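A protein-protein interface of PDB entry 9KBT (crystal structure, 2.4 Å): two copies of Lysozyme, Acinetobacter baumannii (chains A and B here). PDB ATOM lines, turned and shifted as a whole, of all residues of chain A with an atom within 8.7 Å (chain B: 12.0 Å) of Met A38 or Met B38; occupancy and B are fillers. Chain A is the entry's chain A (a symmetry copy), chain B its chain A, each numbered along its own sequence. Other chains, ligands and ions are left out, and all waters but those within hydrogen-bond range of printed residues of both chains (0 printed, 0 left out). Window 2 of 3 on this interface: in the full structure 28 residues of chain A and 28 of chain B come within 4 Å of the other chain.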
ATOM      1  N   ALA A  31       5.363 -11.814   8.637  1.00  0.00           N
ATOM      2  CA  ALA A  31       6.548 -12.662   8.578  1.00  0.00           C
ATOM      3  C   ALA A  31       6.178 -14.128   8.764  1.00  0.00           C
ATOM      4  O   ALA A  31       6.595 -14.990   7.985  1.00  0.00           O
ATOM      5  CB  ALA A  31       7.573 -12.212   9.624  1.00  0.00           C
ATOM      6  N   GLY A  32       5.382 -14.435   9.790  1.00  0.00           N
ATOM      7  CA  GLY A  32       5.089 -15.826  10.092  1.00  0.00           C
ATOM      8  C   GLY A  32       4.198 -16.507   9.071  1.00  0.00           C
ATOM      9  O   GLY A  32       4.338 -17.708   8.829  1.00  0.00           O
ATOM     10  N   ASP A  33       3.244 -15.770   8.492  1.00  0.00           N
ATOM     11  CA  ASP A  33       2.451 -16.295   7.384  1.00  0.00           C
ATOM     12  C   ASP A  33       3.321 -16.558   6.167  1.00  0.00           C
ATOM     13  O   ASP A  33       3.102 -17.532   5.432  1.00  0.00           O
ATOM     14  CB  ASP A  33       1.332 -15.321   7.033  1.00  0.00           C
ATOM     15  CG  ASP A  33       0.305 -15.226   8.137  1.00  0.00           C
ATOM     16  OD1 ASP A  33       0.235 -16.188   8.946  1.00  0.00           O
ATOM     17  OD2 ASP A  33      -0.418 -14.212   8.207  1.00  0.00           O
ATOM     18  N   SER A  34       4.313 -15.703   5.947  1.00  0.00           N
ATOM     19  CA  SER A  34       5.270 -15.960   4.886  1.00  0.00           C
ATOM     20  C   SER A  34       6.039 -17.242   5.150  1.00  0.00           C
ATOM     21  O   SER A  34       6.201 -18.072   4.257  1.00  0.00           O
ATOM     22  CB  SER A  34       6.216 -14.781   4.751  1.00  0.00           C
ATOM     23  OG  SER A  34       7.341 -15.224   4.029  1.00  0.00           O
ATOM     24  N   ILE A  35       6.513 -17.428   6.385  1.00  0.00           N
ATOM     25  CA  ILE A  35       7.220 -18.660   6.729  1.00  0.00           C
ATOM     26  C   ILE A  35       6.316 -19.861   6.535  1.00  0.00           C
ATOM     27  O   ILE A  35       6.743 -20.904   6.019  1.00  0.00           O
ATOM     28  CB  ILE A  35       7.734 -18.612   8.180  1.00  0.00           C
ATOM     29  CG1 ILE A  35       8.977 -17.750   8.286  1.00  0.00           C
ATOM     30  CG2 ILE A  35       7.996 -20.018   8.721  1.00  0.00           C
ATOM     31  CD1 ILE A  35       9.014 -16.988   9.574  1.00  0.00           C
ATOM     32  N   ILE A  36       5.067 -19.755   7.003  1.00  0.00           N
ATOM     33  CA  ILE A  36       4.148 -20.889   6.940  1.00  0.00           C
ATOM     34  C   ILE A  36       3.884 -21.279   5.485  1.00  0.00           C
ATOM     35  O   ILE A  36       3.924 -22.460   5.127  1.00  0.00           O
ATOM     36  CB  ILE A  36       2.843 -20.552   7.677  1.00  0.00           C
ATOM     37  CG1 ILE A  36       3.051 -20.614   9.190  1.00  0.00           C
ATOM     38  CG2 ILE A  36       1.745 -21.484   7.233  1.00  0.00           C
ATOM     39  CD1 ILE A  36       2.024 -19.836   9.953  1.00  0.00           C
ATOM     40  N   ALA A  37       3.628 -20.288   4.626  1.00  0.00           N
ATOM     41  CA  ALA A  37       3.452 -20.523   3.191  1.00  0.00           C
ATOM     42  C   ALA A  37       4.715 -21.080   2.566  1.00  0.00           C
ATOM     43  O   ALA A  37       4.678 -21.996   1.739  1.00  0.00           O
ATOM     44  CB  ALA A  37       3.079 -19.211   2.497  1.00  0.00           C
ATOM     45  N   MET A  38       5.843 -20.554   2.970  1.00  0.00           N
ATOM     46  CA  MET A  38       7.113 -20.950   2.400  1.00  0.00           C
ATOM     47  C   MET A  38       7.659 -22.280   2.966  1.00  0.00           C
ATOM     48  O   MET A  38       8.021 -23.200   2.219  1.00  0.00           O
ATOM     49  CB  MET A  38       8.104 -19.817   2.635  1.00  0.00           C
ATOM     50  CG  MET A  38       9.297 -20.174   1.862  1.00  0.00           C
ATOM     51  SD  MET A  38       8.887 -20.933   0.352  1.00  0.00           S
ATOM     52  CE  MET A  38      10.234 -22.085   0.253  1.00  0.00           C
ATOM     53  N   ASN A  39       7.786 -22.401   4.264  1.00  0.00           N
ATOM     54  CA  ASN A  39       8.500 -23.539   4.811  1.00  0.00           C
ATOM     55  C   ASN A  39       7.583 -24.609   5.361  1.00  0.00           C
ATOM     56  O   ASN A  39       8.002 -25.768   5.438  1.00  0.00           O
ATOM     57  CB  ASN A  39       9.480 -23.088   5.922  1.00  0.00           C
ATOM     58  CG  ASN A  39      10.469 -22.047   5.434  1.00  0.00           C
ATOM     59  OD1 ASN A  39      10.105 -20.885   5.250  1.00  0.00           O
ATOM     60  ND2 ASN A  39      11.722 -22.456   5.205  1.00  0.00           N
ATOM     61  N   GLY A  40       6.344 -24.268   5.718  1.00  0.00           N
ATOM     62  CA  GLY A  40       5.471 -25.207   6.395  1.00  0.00           C
ATOM     63  C   GLY A  40       5.216 -24.809   7.834  1.00  0.00           C
ATOM     64  O   GLY A  40       6.048 -24.146   8.457  1.00  0.00           O
ATOM     65  N   LEU A  41       4.066 -25.211   8.373  1.00  0.00           N
ATOM     66  CA  LEU A  41       3.687 -24.835   9.727  1.00  0.00           C
ATOM     67  C   LEU A  41       4.718 -25.283  10.753  1.00  0.00           C
ATOM     68  O   LEU A  41       4.881 -24.636  11.800  1.00  0.00           O
ATOM     69  CB  LEU A  41       2.330 -25.451  10.046  1.00  0.00           C
ATOM     70  CG  LEU A  41       1.759 -25.250  11.450  1.00  0.00           C
ATOM     71  CD1 LEU A  41       1.781 -23.757  11.857  1.00  0.00           C
ATOM     72  CD2 LEU A  41       0.345 -25.821  11.497  1.00  0.00           C
ATOM     73  N   THR A  43       8.049 -25.418  10.549  1.00  0.00           N
ATOM     74  CA  THR A  43       9.181 -24.509  10.651  1.00  0.00           C
ATOM     75  C   THR A  43       8.815 -23.272  11.450  1.00  0.00           C
ATOM     76  O   THR A  43       9.615 -22.792  12.265  1.00  0.00           O
ATOM     77  CB  THR A  43       9.669 -24.111   9.260  1.00  0.00           C
ATOM     78  OG1 THR A  43      10.176 -25.271   8.602  1.00  0.00           O
ATOM     79  CG2 THR A  43      10.782 -23.058   9.347  1.00  0.00           C
ATOM     80  N   PHE A  44       7.613 -22.737  11.224  1.00  0.00           N
ATOM     81  CA  PHE A  44       7.117 -21.632  12.045  1.00  0.00           C
ATOM     82  C   PHE A  44       7.090 -22.014  13.526  1.00  0.00           C
ATOM     83  O   PHE A  44       7.655 -21.313  14.384  1.00  0.00           O
ATOM     84  CB  PHE A  44       5.728 -21.240  11.571  1.00  0.00           C
ATOM     85  CG  PHE A  44       5.081 -20.162  12.393  1.00  0.00           C
ATOM     86  CD1 PHE A  44       5.742 -18.987  12.674  1.00  0.00           C
ATOM     87  CD2 PHE A  44       3.805 -20.337  12.900  1.00  0.00           C
ATOM     88  CE1 PHE A  44       5.127 -18.009  13.420  1.00  0.00           C
ATOM     89  CE2 PHE A  44       3.192 -19.352  13.625  1.00  0.00           C
ATOM     90  CZ  PHE A  44       3.849 -18.202  13.893  1.00  0.00           C
ATOM     91  N   ASP B   4      20.661  -6.036   5.612  1.00  0.00           N
ATOM     92  CA  ASP B   4      21.078  -7.276   6.251  1.00  0.00           C
ATOM     93  C   ASP B   4      22.585  -7.315   6.466  1.00  0.00           C
ATOM     94  O   ASP B   4      23.364  -6.939   5.585  1.00  0.00           O
ATOM     95  CB  ASP B   4      20.707  -8.482   5.378  1.00  0.00           C
ATOM     96  CG  ASP B   4      19.208  -8.677   5.197  1.00  0.00           C
ATOM     97  OD1 ASP B   4      18.378  -7.934   5.766  1.00  0.00           O
ATOM     98  OD2 ASP B   4      18.864  -9.635   4.488  1.00  0.00           O
ATOM     99  N   ILE B   9      22.971 -12.235  12.638  1.00  0.00           N
ATOM    100  CA  ILE B   9      22.486 -13.600  12.887  1.00  0.00           C
ATOM    101  C   ILE B   9      22.810 -14.043  14.323  1.00  0.00           C
ATOM    102  O   ILE B   9      21.926 -14.439  15.090  1.00  0.00           O
ATOM    103  CB  ILE B   9      23.054 -14.577  11.845  1.00  0.00           C
ATOM    104  CG1 ILE B   9      22.533 -14.220  10.439  1.00  0.00           C
ATOM    105  CG2 ILE B   9      22.663 -15.988  12.169  1.00  0.00           C
ATOM    106  CD1 ILE B   9      23.168 -14.987   9.295  1.00  0.00           C
ATOM    107  N   TYR B  13      19.910 -14.604  17.342  1.00  0.00           N
ATOM    108  CA  TYR B  13      19.835 -15.900  17.990  1.00  0.00           C
ATOM    109  C   TYR B  13      20.032 -15.780  19.490  1.00  0.00           C
ATOM    110  O   TYR B  13      19.302 -16.422  20.247  1.00  0.00           O
ATOM    111  CB  TYR B  13      20.843 -16.860  17.379  1.00  0.00           C
ATOM    112  CG  TYR B  13      20.235 -17.694  16.274  1.00  0.00           C
ATOM    113  CD1 TYR B  13      19.214 -18.597  16.546  1.00  0.00           C
ATOM    114  CD2 TYR B  13      20.658 -17.553  14.949  1.00  0.00           C
ATOM    115  CE1 TYR B  13      18.651 -19.365  15.557  1.00  0.00           C
ATOM    116  CE2 TYR B  13      20.091 -18.315  13.933  1.00  0.00           C
ATOM    117  CZ  TYR B  13      19.096 -19.216  14.249  1.00  0.00           C
ATOM    118  OH  TYR B  13      18.530 -19.961  13.245  1.00  0.00           O
ATOM    119  N   GLN B  28      15.117 -25.280  16.955  1.00  0.00           N
ATOM    120  CA  GLN B  28      14.989 -23.854  16.669  1.00  0.00           C
ATOM    121  C   GLN B  28      16.028 -23.406  15.649  1.00  0.00           C
ATOM    122  O   GLN B  28      15.684 -22.770  14.641  1.00  0.00           O
ATOM    123  CB  GLN B  28      15.164 -23.038  17.939  1.00  0.00           C
ATOM    124  CG  GLN B  28      14.206 -23.305  19.011  1.00  0.00           C
ATOM    125  CD  GLN B  28      14.382 -22.303  20.136  1.00  0.00           C
ATOM    126  OE1 GLN B  28      15.120 -22.556  21.085  1.00  0.00           O
ATOM    127  NE2 GLN B  28      13.729 -21.148  20.019  1.00  0.00           N
ATOM    128  N   VAL B  29      17.318 -23.701  15.920  1.00  0.00           N
ATOM    129  CA  VAL B  29      18.396 -23.240  15.049  1.00  0.00           C
ATOM    130  C   VAL B  29      18.210 -23.775  13.630  1.00  0.00           C
ATOM    131  O   VAL B  29      18.292 -23.028  12.653  1.00  0.00           O
ATOM    132  CB  VAL B  29      19.767 -23.634  15.617  1.00  0.00           C
ATOM    133  CG1 VAL B  29      20.872 -23.144  14.683  1.00  0.00           C
ATOM    134  CG2 VAL B  29      19.954 -23.044  17.002  1.00  0.00           C
ATOM    135  N   THR B  30      17.938 -25.073  13.498  1.00  0.00           N
ATOM    136  CA  THR B  30      17.707 -25.631  12.166  1.00  0.00           C
ATOM    137  C   THR B  30      16.508 -24.975  11.490  1.00  0.00           C
ATOM    138  O   THR B  30      16.546 -24.692  10.282  1.00  0.00           O
ATOM    139  CB  THR B  30      17.501 -27.139  12.268  1.00  0.00           C
ATOM    140  OG1 THR B  30      18.644 -27.730  12.896  1.00  0.00           O
ATOM    141  CG2 THR B  30      17.302 -27.725  10.912  1.00  0.00           C
ATOM    142  N   ALA B  31      15.431 -24.731  12.256  1.00  0.00           N
ATOM    143  CA  ALA B  31      14.283 -24.027  11.695  1.00  0.00           C
ATOM    144  C   ALA B  31      14.667 -22.621  11.254  1.00  0.00           C
ATOM    145  O   ALA B  31      14.364 -22.205  10.132  1.00  0.00           O
ATOM    146  CB  ALA B  31      13.136 -23.995  12.710  1.00  0.00           C
ATOM    147  N   GLY B  32      15.352 -21.872  12.120  1.00  0.00           N
ATOM    148  CA  GLY B  32      15.646 -20.482  11.806  1.00  0.00           C
ATOM    149  C   GLY B  32      16.663 -20.301  10.695  1.00  0.00           C
ATOM    150  O   GLY B  32      16.582 -19.335   9.933  1.00  0.00           O
ATOM    151  N   ASP B  33      17.655 -21.193  10.613  1.00  0.00           N
ATOM    152  CA  ASP B  33      18.581 -21.192   9.483  1.00  0.00           C
ATOM    153  C   ASP B  33      17.860 -21.518   8.186  1.00  0.00           C
ATOM    154  O   ASP B  33      18.184 -20.963   7.126  1.00  0.00           O
ATOM    155  CB  ASP B  33      19.707 -22.191   9.727  1.00  0.00           C
ATOM    156  CG  ASP B  33      20.601 -21.761  10.866  1.00  0.00           C
ATOM    157  OD1 ASP B  33      20.605 -20.539  11.168  1.00  0.00           O
ATOM    158  OD2 ASP B  33      21.285 -22.620  11.457  1.00  0.00           O
ATOM    159  N   SER B  34      16.876 -22.407   8.258  1.00  0.00           N
ATOM    160  CA  SER B  34      16.051 -22.671   7.094  1.00  0.00           C
ATOM    161  C   SER B  34      15.291 -21.424   6.676  1.00  0.00           C
ATOM    162  O   SER B  34      15.251 -21.080   5.496  1.00  0.00           O
ATOM    163  CB  SER B  34      15.095 -23.812   7.390  1.00  0.00           C
ATOM    164  OG  SER B  34      14.070 -23.764   6.426  1.00  0.00           O
ATOM    165  N   ILE B  35      14.687 -20.724   7.639  1.00  0.00           N
ATOM    166  CA  ILE B  35      13.979 -19.486   7.321  1.00  0.00           C
ATOM    167  C   ILE B  35      14.930 -18.472   6.718  1.00  0.00           C
ATOM    168  O   ILE B  35      14.591 -17.776   5.750  1.00  0.00           O
ATOM    169  CB  ILE B  35      13.304 -18.901   8.576  1.00  0.00           C
ATOM    170  CG1 ILE B  35      12.036 -19.659   8.913  1.00  0.00           C
ATOM    171  CG2 ILE B  35      13.020 -17.408   8.407  1.00  0.00           C
ATOM    172  CD1 ILE B  35      11.835 -19.774  10.392  1.00  0.00           C
ATOM    173  N   ILE B  36      16.115 -18.327   7.321  1.00  0.00           N
ATOM    174  CA  ILE B  36      17.065 -17.314   6.867  1.00  0.00           C
ATOM    175  C   ILE B  36      17.500 -17.602   5.429  1.00  0.00           C
ATOM    176  O   ILE B  36      17.531 -16.702   4.583  1.00  0.00           O
ATOM    177  CB  ILE B  36      18.270 -17.256   7.817  1.00  0.00           C
ATOM    178  CG1 ILE B  36      17.896 -16.537   9.112  1.00  0.00           C
ATOM    179  CG2 ILE B  36      19.435 -16.588   7.132  1.00  0.00           C
ATOM    180  CD1 ILE B  36      18.811 -16.869  10.250  1.00  0.00           C
ATOM    181  N   ALA B  37      17.824 -18.864   5.131  1.00  0.00           N
ATOM    182  CA  ALA B  37      18.165 -19.282   3.770  1.00  0.00           C
ATOM    183  C   ALA B  37      16.995 -19.092   2.826  1.00  0.00           C
ATOM    184  O   ALA B  37      17.148 -18.636   1.690  1.00  0.00           O
ATOM    185  CB  ALA B  37      18.579 -20.756   3.774  1.00  0.00           C
ATOM    186  N   MET B  38      15.815 -19.415   3.293  1.00  0.00           N
ATOM    187  CA  MET B  38      14.628 -19.345   2.468  1.00  0.00           C
ATOM    188  C   MET B  38      14.057 -17.917   2.322  1.00  0.00           C
ATOM    189  O   MET B  38      13.805 -17.433   1.210  1.00  0.00           O
ATOM    190  CB  MET B  38      13.587 -20.283   3.068  1.00  0.00           C
ATOM    191  CG  MET B  38      12.498 -20.336   2.088  1.00  0.00           C
ATOM    192  SD  MET B  38      13.093 -20.313   0.456  1.00  0.00           S
ATOM    193  CE  MET B  38      11.797 -19.360  -0.293  1.00  0.00           C
ATOM    194  N   ASN B  39      13.789 -17.238   3.410  1.00  0.00           N
ATOM    195  CA  ASN B  39      13.049 -15.994   3.313  1.00  0.00           C
ATOM    196  C   ASN B  39      13.925 -14.768   3.432  1.00  0.00           C
ATOM    197  O   ASN B  39      13.531 -13.706   2.941  1.00  0.00           O
ATOM    198  CB  ASN B  39      11.939 -15.933   4.393  1.00  0.00           C
ATOM    199  CG  ASN B  39      10.984 -17.107   4.308  1.00  0.00           C
ATOM    200  OD1 ASN B  39      11.335 -18.221   4.699  1.00  0.00           O
ATOM    201  ND2 ASN B  39       9.776 -16.875   3.784  1.00  0.00           N
ATOM    202  N   GLY B  40      15.108 -14.883   4.039  1.00  0.00           N
ATOM    203  CA  GLY B  40      15.924 -13.719   4.323  1.00  0.00           C
ATOM    204  C   GLY B  40      16.006 -13.433   5.808  1.00  0.00           C
ATOM    205  O   GLY B  40      15.093 -13.773   6.563  1.00  0.00           O
ATOM    206  N   LEU B  41      17.099 -12.804   6.239  1.00  0.00           N
ATOM    207  CA  LEU B  41      17.315 -12.532   7.651  1.00  0.00           C
ATOM    208  C   LEU B  41      16.188 -11.703   8.252  1.00  0.00           C
ATOM    209  O   LEU B  41      15.892 -11.825   9.451  1.00  0.00           O
ATOM    210  CB  LEU B  41      18.644 -11.803   7.814  1.00  0.00           C
ATOM    211  CG  LEU B  41      19.048 -11.347   9.217  1.00  0.00           C
ATOM    212  CD1 LEU B  41      18.942 -12.506  10.237  1.00  0.00           C
ATOM    213  CD2 LEU B  41      20.463 -10.778   9.164  1.00  0.00           C
ATOM    214  N   LYS B  42      15.554 -10.844   7.448  1.00  0.00           N
ATOM    215  CA  LYS B  42      14.529  -9.968   7.999  1.00  0.00           C
ATOM    216  C   LYS B  42      13.289 -10.753   8.418  1.00  0.00           C
ATOM    217  O   LYS B  42      12.686 -10.464   9.460  1.00  0.00           O
ATOM    218  CB  LYS B  42      14.170  -8.884   6.988  1.00  0.00           C
ATOM    219  CG  LYS B  42      14.857  -7.559   7.242  1.00  0.00           C
ATOM    220  CD  LYS B  42      14.479  -6.568   6.162  1.00  0.00           C
ATOM    221  CE  LYS B  42      14.792  -7.105   4.742  1.00  0.00           C
ATOM    222  NZ  LYS B  42      16.198  -6.829   4.268  1.00  0.00           N
ATOM    223  N   THR B  43      12.905 -11.759   7.638  1.00  0.00           N
ATOM    224  CA  THR B  43      11.746 -12.559   8.005  1.00  0.00           C
ATOM    225  C   THR B  43      11.987 -13.305   9.304  1.00  0.00           C
ATOM    226  O   THR B  43      11.089 -13.396  10.152  1.00  0.00           O
ATOM    227  CB  THR B  43      11.405 -13.543   6.889  1.00  0.00           C
ATOM    228  OG1 THR B  43      11.005 -12.809   5.734  1.00  0.00           O
ATOM    229  CG2 THR B  43      10.262 -14.479   7.308  1.00  0.00           C
ATOM    230  N   PHE B  44      13.192 -13.853   9.474  1.00  0.00           N
ATOM    231  CA  PHE B  44      13.565 -14.467  10.749  1.00  0.00           C
ATOM    232  C   PHE B  44      13.437 -13.469  11.901  1.00  0.00           C
ATOM    233  O   PHE B  44      12.761 -13.733  12.911  1.00  0.00           O
ATOM    234  CB  PHE B  44      14.987 -14.992  10.656  1.00  0.00           C
ATOM    235  CG  PHE B  44      15.510 -15.579  11.936  1.00  0.00           C
ATOM    236  CD1 PHE B  44      14.791 -16.524  12.632  1.00  0.00           C
ATOM    237  CD2 PHE B  44      16.726 -15.163  12.453  1.00  0.00           C
ATOM    238  CE1 PHE B  44      15.293 -17.055  13.797  1.00  0.00           C
ATOM    239  CE2 PHE B  44      17.228 -15.710  13.602  1.00  0.00           C
ATOM    240  CZ  PHE B  44      16.515 -16.639  14.275  1.00  0.00           C
ATOM    241  N   ALA B  45      14.078 -12.309  11.772  1.00  0.00           N
ATOM    242  CA  ALA B  45      14.041 -11.361  12.876  1.00  0.00           C
ATOM    243  C   ALA B  45      12.620 -10.876  13.144  1.00  0.00           C
ATOM    244  O   ALA B  45      12.257 -10.596  14.296  1.00  0.00           O
ATOM    245  CB  ALA B  45      14.968 -10.184  12.585  1.00  0.00           C
ATOM    246  N   GLN B  46      11.795 -10.795  12.105  1.00  0.00           N
ATOM    247  CA  GLN B  46      10.506 -10.162  12.310  1.00  0.00           C
ATOM    248  C   GLN B  46       9.537 -11.089  13.027  1.00  0.00           C
ATOM    249  O   GLN B  46       8.744 -10.634  13.865  1.00  0.00           O
ATOM    250  CB  GLN B  46       9.925  -9.720  10.981  1.00  0.00           C
ATOM    251  CG  GLN B  46      10.484  -8.424  10.519  1.00  0.00           C
ATOM    252  CD  GLN B  46      10.165  -8.167   9.079  1.00  0.00           C
ATOM    253  OE1 GLN B  46       9.705  -9.065   8.359  1.00  0.00           O
ATOM    254  NE2 GLN B  46      10.399  -6.946   8.638  1.00  0.00           N
ATOM    255  N   VAL B  47       9.588 -12.386  12.711  1.00  0.00           N
ATOM    256  CA  VAL B  47       8.570 -13.280  13.236  1.00  0.00           C
ATOM    257  C   VAL B  47       8.794 -13.511  14.722  1.00  0.00           C
ATOM    258  O   VAL B  47       7.833 -13.715  15.472  1.00  0.00           O
ATOM    259  CB  VAL B  47       8.551 -14.604  12.465  1.00  0.00           C
ATOM    260  CG1 VAL B  47       9.889 -15.315  12.614  1.00  0.00           C
ATOM    261  CG2 VAL B  47       7.437 -15.464  12.997  1.00  0.00           C
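The side-chain amide oxygen of Asn A39 sits close to the side-chain amide oxygen of Asn B39, 3.0 Å away.
ND2 of Asn B39 is in hydrogen-bond range of OG of Ser A34.
The side-chain hydroxyl of Ser B34 sits at hydrogen-bond distance from the side-chain amide nitrogen of Asn A39 (3.0 Å).
OD1 of Asn B39 sits close to O of Ile B35 (3.5 Å).
O of Ile A35 sits close to OD1 of Asn A39, 3.4 Å away.
O of Lys B42 sits close to OE1 of Gln B46 (3.5 Å).
O of Ile B35 sits at hydrogen-bond distance from N of Gly B40 (3.4 Å).
The backbone carbonyl oxygen (O) of Ile A35 sits at hydrogen-bond distance from the backbone NH (N) of Gly A40 (3.4 Å).
Among the printed residues, merely in contact across the chains: Met A38 with Met B38, Phe A44 with Val B47, Asn A39 with Met B38, Met A38 with Asn B39, Ile A35 with Val B47, Thr A43 with Ile B35, Ile A35 with Thr B43, Ile A35 with Ile B35, Ala A31 with Gln B46, Ala A31 with Val B47, Thr A43 with Ala B31, Ala A31 with Thr B43 and Gly A32 with Val B47.
Printed residues of chain B within 4 Å of Gly A32: Val B47 (3.8 Å).
Of chain B, only Asn B39 (3.0 Å) comes within 4 Å of Ser A34.
Of the printed residues of chain B, Ile A35 touches Ile B35, Thr B43 and Val B47.
Met A38 touches two residues of chain B.
Asn A39 touches just these residues of chain B: Ser B34 (3.0 Å), Met B38 (3.6 Å) and Asn B39 (3.0 Å).
No residue of chain B comes within 4 Å of Gly A40.
Thr B30 touches none of the printed residues of chain A.
Asp B33 touches none of the printed residues of chain A.
Printed residues of chain A within 4 Å of Ser B34: Asn A39 (3.0 Å).
Of chain A, only Met A38 and Asn A39 come within 4 Å of Met B38.
Asn B39 touches three residues of chain A.
The nearest residue of chain A that does not touch Met B38 is Ile A35 (7.0 Å).
The nearest printed residue of chain A that does not touch Gln B46 is Gly A32 (6.2 Å).
Printed residues of chain B that touch a printed residue of chain A: Ala B31, Ser B34, Ile B35, Met B38, Asn B39, Thr B43, Gln B46 and Val B47.
Of the 13 printed residues of chain A, 8 touch a printed residue of chain B.
Among the printed residues, 16 pairs touch across the chains.
Among the printed residues, no Asp or Glu carboxylate lies within 4 Å of a Lys or Arg side-chain nitrogen of the other chain.
Ser A34 touches Asn B39, and with the chains exchanged Asn A39 touches Ser B34.
Ile A35 touches its own counterpart, Ile B35.
Met A38 touches its own counterpart, Met B38.
Asn A39 touches its own counterpart, Asn B39.
Of the 16 pairs that touch across the chains among the printed residues, 11 have their exchanged pair printed and touching as well.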
